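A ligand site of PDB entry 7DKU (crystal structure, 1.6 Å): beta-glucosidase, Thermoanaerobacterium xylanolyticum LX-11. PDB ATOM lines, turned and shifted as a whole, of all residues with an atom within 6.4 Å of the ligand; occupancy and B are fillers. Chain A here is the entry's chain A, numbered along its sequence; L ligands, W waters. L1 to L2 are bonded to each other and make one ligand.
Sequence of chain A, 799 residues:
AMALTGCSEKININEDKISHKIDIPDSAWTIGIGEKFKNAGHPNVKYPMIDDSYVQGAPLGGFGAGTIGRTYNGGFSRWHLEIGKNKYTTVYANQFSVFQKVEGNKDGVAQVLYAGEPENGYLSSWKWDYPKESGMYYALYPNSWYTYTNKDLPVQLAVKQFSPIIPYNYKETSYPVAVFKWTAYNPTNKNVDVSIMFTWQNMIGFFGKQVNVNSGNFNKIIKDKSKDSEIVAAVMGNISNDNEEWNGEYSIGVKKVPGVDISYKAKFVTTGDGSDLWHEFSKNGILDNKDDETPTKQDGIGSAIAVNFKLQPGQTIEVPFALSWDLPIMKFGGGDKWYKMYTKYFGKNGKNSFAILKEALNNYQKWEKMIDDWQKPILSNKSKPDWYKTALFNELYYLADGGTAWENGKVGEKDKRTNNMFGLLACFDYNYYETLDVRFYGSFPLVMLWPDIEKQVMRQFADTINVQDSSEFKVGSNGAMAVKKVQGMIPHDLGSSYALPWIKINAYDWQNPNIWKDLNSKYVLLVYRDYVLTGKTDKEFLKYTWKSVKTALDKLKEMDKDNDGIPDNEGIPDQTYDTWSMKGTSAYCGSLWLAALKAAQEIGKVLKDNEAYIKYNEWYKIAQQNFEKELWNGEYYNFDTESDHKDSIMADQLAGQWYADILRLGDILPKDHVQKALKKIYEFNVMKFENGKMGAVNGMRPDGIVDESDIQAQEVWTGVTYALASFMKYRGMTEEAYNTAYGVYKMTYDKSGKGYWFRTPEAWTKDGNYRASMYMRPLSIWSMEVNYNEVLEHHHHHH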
ATOM      1  N   TYR A  47      18.251  26.088   9.936  1.00  0.00           N
ATOM      2  CA  TYR A  47      17.224  27.076  10.221  1.00  0.00           C
ATOM      3  C   TYR A  47      17.639  28.395   9.548  1.00  0.00           C
ATOM      4  O   TYR A  47      18.810  28.541   9.195  1.00  0.00           O
ATOM      5  CB  TYR A  47      16.951  27.213  11.728  1.00  0.00           C
ATOM      6  CG  TYR A  47      18.156  27.481  12.579  1.00  0.00           C
ATOM      7  CD1 TYR A  47      18.949  26.440  13.064  1.00  0.00           C
ATOM      8  CD2 TYR A  47      18.532  28.783  12.900  1.00  0.00           C
ATOM      9  CE1 TYR A  47      20.070  26.681  13.856  1.00  0.00           C
ATOM     10  CE2 TYR A  47      19.633  29.038  13.690  1.00  0.00           C
ATOM     11  CZ  TYR A  47      20.410  27.994  14.157  1.00  0.00           C
ATOM     12  OH  TYR A  47      21.517  28.219  14.938  1.00  0.00           O
ATOM     13  N   ASP A 429      20.839  37.343  14.988  1.00  0.00           N
ATOM     14  CA  ASP A 429      20.136  36.052  14.902  1.00  0.00           C
ATOM     15  C   ASP A 429      19.630  35.592  16.260  1.00  0.00           C
ATOM     16  O   ASP A 429      18.540  35.008  16.354  1.00  0.00           O
ATOM     17  CB  ASP A 429      21.030  34.960  14.336  1.00  0.00           C
ATOM     18  CG  ASP A 429      21.394  35.183  12.878  1.00  0.00           C
ATOM     19  OD1 ASP A 429      20.515  35.053  11.995  1.00  0.00           O
ATOM     20  OD2 ASP A 429      22.578  35.452  12.609  1.00  0.00           O
ATOM     21  N   TYR A 430      20.416  35.825  17.294  1.00  0.00           N
ATOM     22  CA  TYR A 430      20.085  35.512  18.675  1.00  0.00           C
ATOM     23  C   TYR A 430      20.034  36.850  19.414  1.00  0.00           C
ATOM     24  O   TYR A 430      21.039  37.306  19.975  1.00  0.00           O
ATOM     25  CB  TYR A 430      21.132  34.572  19.288  1.00  0.00           C
ATOM     26  CG  TYR A 430      21.587  33.402  18.427  1.00  0.00           C
ATOM     27  CD1 TYR A 430      20.687  32.629  17.698  1.00  0.00           C
ATOM     28  CD2 TYR A 430      22.925  33.012  18.409  1.00  0.00           C
ATOM     29  CE1 TYR A 430      21.125  31.531  16.937  1.00  0.00           C
ATOM     30  CE2 TYR A 430      23.362  31.939  17.676  1.00  0.00           C
ATOM     31  CZ  TYR A 430      22.472  31.187  16.940  1.00  0.00           C
ATOM     32  OH  TYR A 430      22.955  30.104  16.223  1.00  0.00           O
ATOM     33  N   TYR A 432      19.644  38.985  21.804  1.00  0.00           N
ATOM     34  CA  TYR A 432      19.679  39.078  23.267  1.00  0.00           C
ATOM     35  C   TYR A 432      20.712  40.126  23.711  1.00  0.00           C
ATOM     36  O   TYR A 432      21.883  40.045  23.308  1.00  0.00           O
ATOM     37  CB  TYR A 432      19.976  37.703  23.887  1.00  0.00           C
ATOM     38  CG  TYR A 432      19.022  36.653  23.356  1.00  0.00           C
ATOM     39  CD1 TYR A 432      17.654  36.833  23.497  1.00  0.00           C
ATOM     40  CD2 TYR A 432      19.476  35.510  22.696  1.00  0.00           C
ATOM     41  CE1 TYR A 432      16.758  35.903  22.994  1.00  0.00           C
ATOM     42  CE2 TYR A 432      18.580  34.581  22.192  1.00  0.00           C
ATOM     43  CZ  TYR A 432      17.216  34.789  22.340  1.00  0.00           C
ATOM     44  OH  TYR A 432      16.313  33.855  21.815  1.00  0.00           O
ATOM     45  N   HIS A 492      20.988  35.230  31.991  1.00  0.00           N
ATOM     46  CA  HIS A 492      21.697  35.059  30.728  1.00  0.00           C
ATOM     47  C   HIS A 492      21.833  36.377  29.961  1.00  0.00           C
ATOM     48  O   HIS A 492      22.882  36.630  29.350  1.00  0.00           O
ATOM     49  CB  HIS A 492      20.922  34.048  29.879  1.00  0.00           C
ATOM     50  CG  HIS A 492      21.483  33.850  28.510  1.00  0.00           C
ATOM     51  ND1 HIS A 492      21.051  34.575  27.421  1.00  0.00           N
ATOM     52  CD2 HIS A 492      22.422  32.999  28.040  1.00  0.00           C
ATOM     53  CE1 HIS A 492      21.695  34.185  26.342  1.00  0.00           C
ATOM     54  NE2 HIS A 492      22.525  33.223  26.687  1.00  0.00           N
ATOM     55  N   TYR A 508      16.387  34.806  26.320  1.00  0.00           N
ATOM     56  CA  TYR A 508      16.887  33.520  25.845  1.00  0.00           C
ATOM     57  C   TYR A 508      16.149  32.356  26.489  1.00  0.00           C
ATOM     58  O   TYR A 508      15.938  32.354  27.706  1.00  0.00           O
ATOM     59  CB  TYR A 508      18.388  33.456  26.159  1.00  0.00           C
ATOM     60  CG  TYR A 508      19.083  32.131  25.962  1.00  0.00           C
ATOM     61  CD1 TYR A 508      19.198  31.229  27.017  1.00  0.00           C
ATOM     62  CD2 TYR A 508      19.717  31.810  24.765  1.00  0.00           C
ATOM     63  CE1 TYR A 508      19.891  30.056  26.883  1.00  0.00           C
ATOM     64  CE2 TYR A 508      20.426  30.616  24.620  1.00  0.00           C
ATOM     65  CZ  TYR A 508      20.483  29.731  25.685  1.00  0.00           C
ATOM     66  OH  TYR A 508      21.148  28.550  25.600  1.00  0.00           O
ATOM     67  N   ASP A 509      15.752  31.400  25.667  1.00  0.00           N
ATOM     68  CA  ASP A 509      15.007  30.223  26.148  1.00  0.00           C
ATOM     69  C   ASP A 509      15.457  28.891  25.588  1.00  0.00           C
ATOM     70  O   ASP A 509      14.820  27.869  25.867  1.00  0.00           O
ATOM     71  CB  ASP A 509      13.494  30.420  25.938  1.00  0.00           C
ATOM     72  CG  ASP A 509      13.118  30.630  24.490  1.00  0.00           C
ATOM     73  OD1 ASP A 509      13.954  30.442  23.584  1.00  0.00           O
ATOM     74  OD2 ASP A 509      11.947  31.001  24.263  1.00  0.00           O
ATOM     75  N   TRP A 510      16.557  28.850  24.830  1.00  0.00           N
ATOM     76  CA  TRP A 510      17.039  27.588  24.259  1.00  0.00           C
ATOM     77  C   TRP A 510      17.432  26.576  25.357  1.00  0.00           C
ATOM     78  O   TRP A 510      17.168  25.375  25.247  1.00  0.00           O
ATOM     79  CB  TRP A 510      18.204  27.833  23.302  1.00  0.00           C
ATOM     80  CG  TRP A 510      18.859  26.592  22.849  1.00  0.00           C
ATOM     81  CD1 TRP A 510      20.115  26.180  23.159  1.00  0.00           C
ATOM     82  CD2 TRP A 510      18.287  25.572  22.048  1.00  0.00           C
ATOM     83  NE1 TRP A 510      20.379  24.972  22.578  1.00  0.00           N
ATOM     84  CE2 TRP A 510      19.267  24.571  21.890  1.00  0.00           C
ATOM     85  CE3 TRP A 510      17.026  25.401  21.442  1.00  0.00           C
ATOM     86  CZ2 TRP A 510      19.036  23.407  21.148  1.00  0.00           C
ATOM     87  CZ3 TRP A 510      16.805  24.236  20.697  1.00  0.00           C
ATOM     88  CH2 TRP A 510      17.802  23.261  20.553  1.00  0.00           C
ATOM     89  N   THR A 576      27.837  28.338  28.360  1.00  0.00           N
ATOM     90  CA  THR A 576      27.887  29.043  27.066  1.00  0.00           C
ATOM     91  C   THR A 576      27.947  28.148  25.832  1.00  0.00           C
ATOM     92  O   THR A 576      27.407  28.507  24.782  1.00  0.00           O
ATOM     93  CB  THR A 576      29.065  30.059  27.021  1.00  0.00           C
ATOM     94  OG1 THR A 576      28.815  31.060  26.019  1.00  0.00           O
ATOM     95  CG2 THR A 576      30.403  29.397  26.790  1.00  0.00           C
ATOM     96  N   ASP A 578      26.215  25.928  24.517  1.00  0.00           N
ATOM     97  CA  ASP A 578      24.852  25.584  24.903  1.00  0.00           C
ATOM     98  C   ASP A 578      24.211  24.466  24.073  1.00  0.00           C
ATOM     99  O   ASP A 578      23.002  24.238  24.178  1.00  0.00           O
ATOM    100  CB  ASP A 578      23.958  26.819  24.981  1.00  0.00           C
ATOM    101  CG  ASP A 578      23.752  27.510  23.637  1.00  0.00           C
ATOM    102  OD1 ASP A 578      24.516  27.261  22.680  1.00  0.00           O
ATOM    103  OD2 ASP A 578      22.821  28.335  23.583  1.00  0.00           O
ATOM    104  N   THR A 579      25.008  23.786  23.259  1.00  0.00           N
ATOM    105  CA  THR A 579      24.619  22.472  22.725  1.00  0.00           C
ATOM    106  C   THR A 579      25.633  21.367  23.088  1.00  0.00           C
ATOM    107  O   THR A 579      25.415  20.204  22.739  1.00  0.00           O
ATOM    108  CB  THR A 579      24.295  22.503  21.214  1.00  0.00           C
ATOM    109  OG1 THR A 579      25.447  22.889  20.460  1.00  0.00           O
ATOM    110  CG2 THR A 579      23.135  23.446  20.924  1.00  0.00           C
ATOM    111  N   ILE A 711      28.172  19.510  17.426  1.00  0.00           N
ATOM    112  CA  ILE A 711      28.585  20.544  16.462  1.00  0.00           C
ATOM    113  C   ILE A 711      29.522  21.598  17.074  1.00  0.00           C
ATOM    114  O   ILE A 711      30.498  21.982  16.432  1.00  0.00           O
ATOM    115  CB  ILE A 711      27.339  21.232  15.805  1.00  0.00           C
ATOM    116  CG1 ILE A 711      27.758  22.249  14.728  1.00  0.00           C
ATOM    117  CG2 ILE A 711      26.430  21.885  16.846  1.00  0.00           C
ATOM    118  CD1 ILE A 711      28.610  21.660  13.623  1.00  0.00           C
ATOM    119  N   GLN A 712      29.259  22.037  18.295  1.00  0.00           N
ATOM    120  CA  GLN A 712      30.101  23.095  18.902  1.00  0.00           C
ATOM    121  C   GLN A 712      31.524  22.632  19.152  1.00  0.00           C
ATOM    122  O   GLN A 712      32.458  23.441  19.076  1.00  0.00           O
ATOM    123  CB  GLN A 712      29.484  23.656  20.170  1.00  0.00           C
ATOM    124  CG  GLN A 712      28.254  24.494  19.882  1.00  0.00           C
ATOM    125  CD  GLN A 712      27.514  24.934  21.119  1.00  0.00           C
ATOM    126  OE1 GLN A 712      27.745  24.419  22.224  1.00  0.00           O
ATOM    127  NE2 GLN A 712      26.611  25.885  20.952  1.00  0.00           N
ATOM    128  N   TRP A 717      35.437  28.952  17.624  1.00  0.00           N
ATOM    129  CA  TRP A 717      34.745  30.148  18.108  1.00  0.00           C
ATOM    130  C   TRP A 717      35.742  31.284  18.060  1.00  0.00           C
ATOM    131  O   TRP A 717      36.776  31.221  18.698  1.00  0.00           O
ATOM    132  CB  TRP A 717      34.169  29.935  19.520  1.00  0.00           C
ATOM    133  CG  TRP A 717      32.897  29.119  19.517  1.00  0.00           C
ATOM    134  CD1 TRP A 717      32.438  28.303  18.525  1.00  0.00           C
ATOM    135  CD2 TRP A 717      31.931  29.030  20.578  1.00  0.00           C
ATOM    136  NE1 TRP A 717      31.261  27.720  18.890  1.00  0.00           N
ATOM    137  CE2 TRP A 717      30.923  28.153  20.141  1.00  0.00           C
ATOM    138  CE3 TRP A 717      31.839  29.599  21.851  1.00  0.00           C
ATOM    139  CZ2 TRP A 717      29.813  27.842  20.948  1.00  0.00           C
ATOM    140  CZ3 TRP A 717      30.725  29.293  22.639  1.00  0.00           C
ATOM    141  CH2 TRP A 717      29.730  28.420  22.178  1.00  0.00           C
ATOM    142  N   GLU A 762      30.212  34.205  15.244  1.00  0.00           N
ATOM    143  CA  GLU A 762      30.549  33.387  16.388  1.00  0.00           C
ATOM    144  C   GLU A 762      31.555  32.304  15.987  1.00  0.00           C
ATOM    145  O   GLU A 762      32.590  32.116  16.623  1.00  0.00           O
ATOM    146  CB  GLU A 762      29.297  32.722  16.978  1.00  0.00           C
ATOM    147  CG  GLU A 762      29.555  31.612  18.001  1.00  0.00           C
ATOM    148  CD  GLU A 762      29.700  32.093  19.421  1.00  0.00           C
ATOM    149  OE1 GLU A 762      30.736  32.707  19.768  1.00  0.00           O
ATOM    150  OE2 GLU A 762      28.783  31.838  20.230  1.00  0.00           O
ATOM    151  N   ARG A 771      28.374  30.246  11.603  1.00  0.00           N
ATOM    152  CA  ARG A 771      27.157  30.410  12.395  1.00  0.00           C
ATOM    153  C   ARG A 771      27.197  31.768  13.082  1.00  0.00           C
ATOM    154  O   ARG A 771      28.186  32.107  13.755  1.00  0.00           O
ATOM    155  CB  ARG A 771      27.044  29.295  13.435  1.00  0.00           C
ATOM    156  CG  ARG A 771      25.738  29.321  14.204  1.00  0.00           C
ATOM    157  CD  ARG A 771      25.538  28.025  14.962  1.00  0.00           C
ATOM    158  NE  ARG A 771      26.569  27.791  15.984  1.00  0.00           N
ATOM    159  CZ  ARG A 771      26.535  28.244  17.231  1.00  0.00           C
ATOM    160  NH1 ARG A 771      25.535  29.021  17.656  1.00  0.00           N
ATOM    161  NH2 ARG A 771      27.527  27.955  18.066  1.00  0.00           N
ATOM    162  N   TYR A 775      28.809  39.242  15.448  1.00  0.00           N
ATOM    163  CA  TYR A 775      28.784  38.608  16.775  1.00  0.00           C
ATOM    164  C   TYR A 775      29.650  39.343  17.782  1.00  0.00           C
ATOM    165  O   TYR A 775      30.705  39.842  17.450  1.00  0.00           O
ATOM    166  CB  TYR A 775      29.228  37.148  16.644  1.00  0.00           C
ATOM    167  CG  TYR A 775      28.638  36.280  17.712  1.00  0.00           C
ATOM    168  CD1 TYR A 775      27.317  35.863  17.626  1.00  0.00           C
ATOM    169  CD2 TYR A 775      29.366  35.909  18.836  1.00  0.00           C
ATOM    170  CE1 TYR A 775      26.745  35.077  18.594  1.00  0.00           C
ATOM    171  CE2 TYR A 775      28.795  35.137  19.839  1.00  0.00           C
ATOM    172  CZ  TYR A 775      27.472  34.719  19.710  1.00  0.00           C
ATOM    173  OH  TYR A 775      26.910  33.946  20.710  1.00  0.00           O
HETATM  174  C1  LIG L   1      16.424  26.123  17.364  1.00  0.00           C
HETATM  175  C2  LIG L   1      17.671  26.994  17.550  1.00  0.00           C
HETATM  176  C3  LIG L   1      18.830  26.106  17.963  1.00  0.00           C
HETATM  177  C4  LIG L   1      18.969  24.871  17.077  1.00  0.00           C
HETATM  178  C5  LIG L   1      19.968  23.864  17.610  1.00  0.00           C
HETATM  179  C6  LIG L   1      16.723  25.002  16.389  1.00  0.00           C
HETATM  180  O1  LIG L   1      15.589  24.157  16.157  1.00  0.00           O
HETATM  181  O2  LIG L   1      15.349  26.915  16.870  1.00  0.00           O
HETATM  182  O3  LIG L   1      17.444  27.997  18.549  1.00  0.00           O
HETATM  183  O4  LIG L   1      20.079  26.808  17.846  1.00  0.00           O
HETATM  184  O5  LIG L   1      17.719  24.189  16.975  1.00  0.00           O
HETATM  185  O6  LIG L   1      20.191  22.844  16.640  1.00  0.00           O
HETATM  186  C1  LG2 L   2      22.073  27.448  18.941  1.00  0.00           C
HETATM  187  C2  LG2 L   2      22.605  28.050  20.231  1.00  0.00           C
HETATM  188  C3  LG2 L   2      21.954  29.408  20.392  1.00  0.00           C
HETATM  189  C4  LG2 L   2      20.421  29.269  20.440  1.00  0.00           C
HETATM  190  C5  LG2 L   2      19.705  30.599  20.634  1.00  0.00           C
HETATM  191  C6  LG2 L   2      20.563  27.352  19.058  1.00  0.00           C
HETATM  192  O1  LG2 L   2      22.625  26.149  18.716  1.00  0.00           O
HETATM  193  O2  LG2 L   2      24.039  28.120  20.181  1.00  0.00           O
HETATM  194  O3  LG2 L   2      22.410  30.020  21.598  1.00  0.00           O
HETATM  195  O4  LG2 L   2      19.984  28.635  19.233  1.00  0.00           O
HETATM  196  O5  LG2 L   2      18.288  30.390  20.598  1.00  0.00           O
HETATM  197  O   HOH W   1      16.767  31.233  22.763  1.00  0.00           O
HETATM  198  O   HOH W   2      27.025  29.757  20.301  1.00  0.00           O
HETATM  199  O   HOH W   3      15.771  28.413  14.742  1.00  0.00           O
HETATM  200  O   HOH W   4      22.874  22.627  17.129  1.00  0.00           O
HETATM  201  O   HOH W   5      22.625  26.066  15.969  1.00  0.00           O
HETATM  202  O   HOH W   6      17.235  32.598  19.385  1.00  0.00           O
HETATM  203  O   HOH W   7      25.073  24.969  18.400  1.00  0.00           O
HETATM  204  O   HOH W   8      19.222  22.783  14.074  1.00  0.00           O
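The side-chain carboxylate (OD2) of Asp 578 sits at hydrogen-bond distance from an oxygen (O3) of LG2 L2 (2.6 Å). The guanidinium group of Arg 771 is in hydrogen-bond range of an oxygen (O2) of LG2 L2. An oxygen (O2) of LG2 L2 lies within hydrogen-bond range of the side-chain amide nitrogen (NE2) of Gln 712, 3.5 Å away.
The backbone NH (N) of Thr 579 sits at hydrogen-bond distance from the side-chain amide oxygen (OE1) of Gln 712, 3.0 Å away. The backbone carbonyl oxygen of Asp 578 is in hydrogen-bond range of the indole nitrogen of Trp 510. The side-chain amide nitrogen of Gln 712 sits at hydrogen-bond distance from the side-chain carboxylate of Asp 578. OH of Tyr 508 sits at hydrogen-bond distance from OD2 of Asp 578, at 2.6 Å. The guanidinium group of Arg 771 sits at hydrogen-bond distance from the side-chain hydroxyl of Tyr 430, at 3.1 Å. The backbone carbonyl oxygen (O) of Arg 771 lies within hydrogen-bond range of the backbone NH (N) of Glu 762, at 3.3 Å. The side-chain hydroxyl of Tyr 47 is in hydrogen-bond range of the side-chain hydroxyl of Tyr 430 (2.7 Å).
Merely in contact with the ligand: Thr 579 (3.5 Å), Tyr 47 (3.5 Å), Tyr 508 (3.7 Å), Trp 510 (3.7 Å) and Tyr 430 (3.7 Å). Within 4 Å of the ligand: Tyr 47, Tyr 430, Tyr 508, Trp 510, Asp 578, Thr 579, Gln 712 and Arg 771.
Water W6 lies within hydrogen-bond range of O5 of LG2 L2 (2.7 Å) and OH of Tyr 432 (2.9 Å). Water W7 lies within hydrogen-bond range of O1 of LG2 L2, OG1 of Thr 579 and NE2 of Gln 712. Water W5 bridges OH of Tyr 47 and O1 of LG2 L2. Water W1 lies within hydrogen-bond range of an oxygen (O5) of LG2 L2 (2.8 Å), the side-chain hydroxyl (OH) of Tyr 432 (2.8 Å), the side-chain carboxylate (OD1) of Asp 509 (3.0 Å) and the backbone NH (N) of Trp 510 (3.2 Å). Water W2 lies within hydrogen-bond range of the side-chain carboxylate of Glu 762 (2.7 Å), the guanidinium group of Arg 771 (2.9 Å) and an oxygen (O2) of LG2 L2 (3.4 Å).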
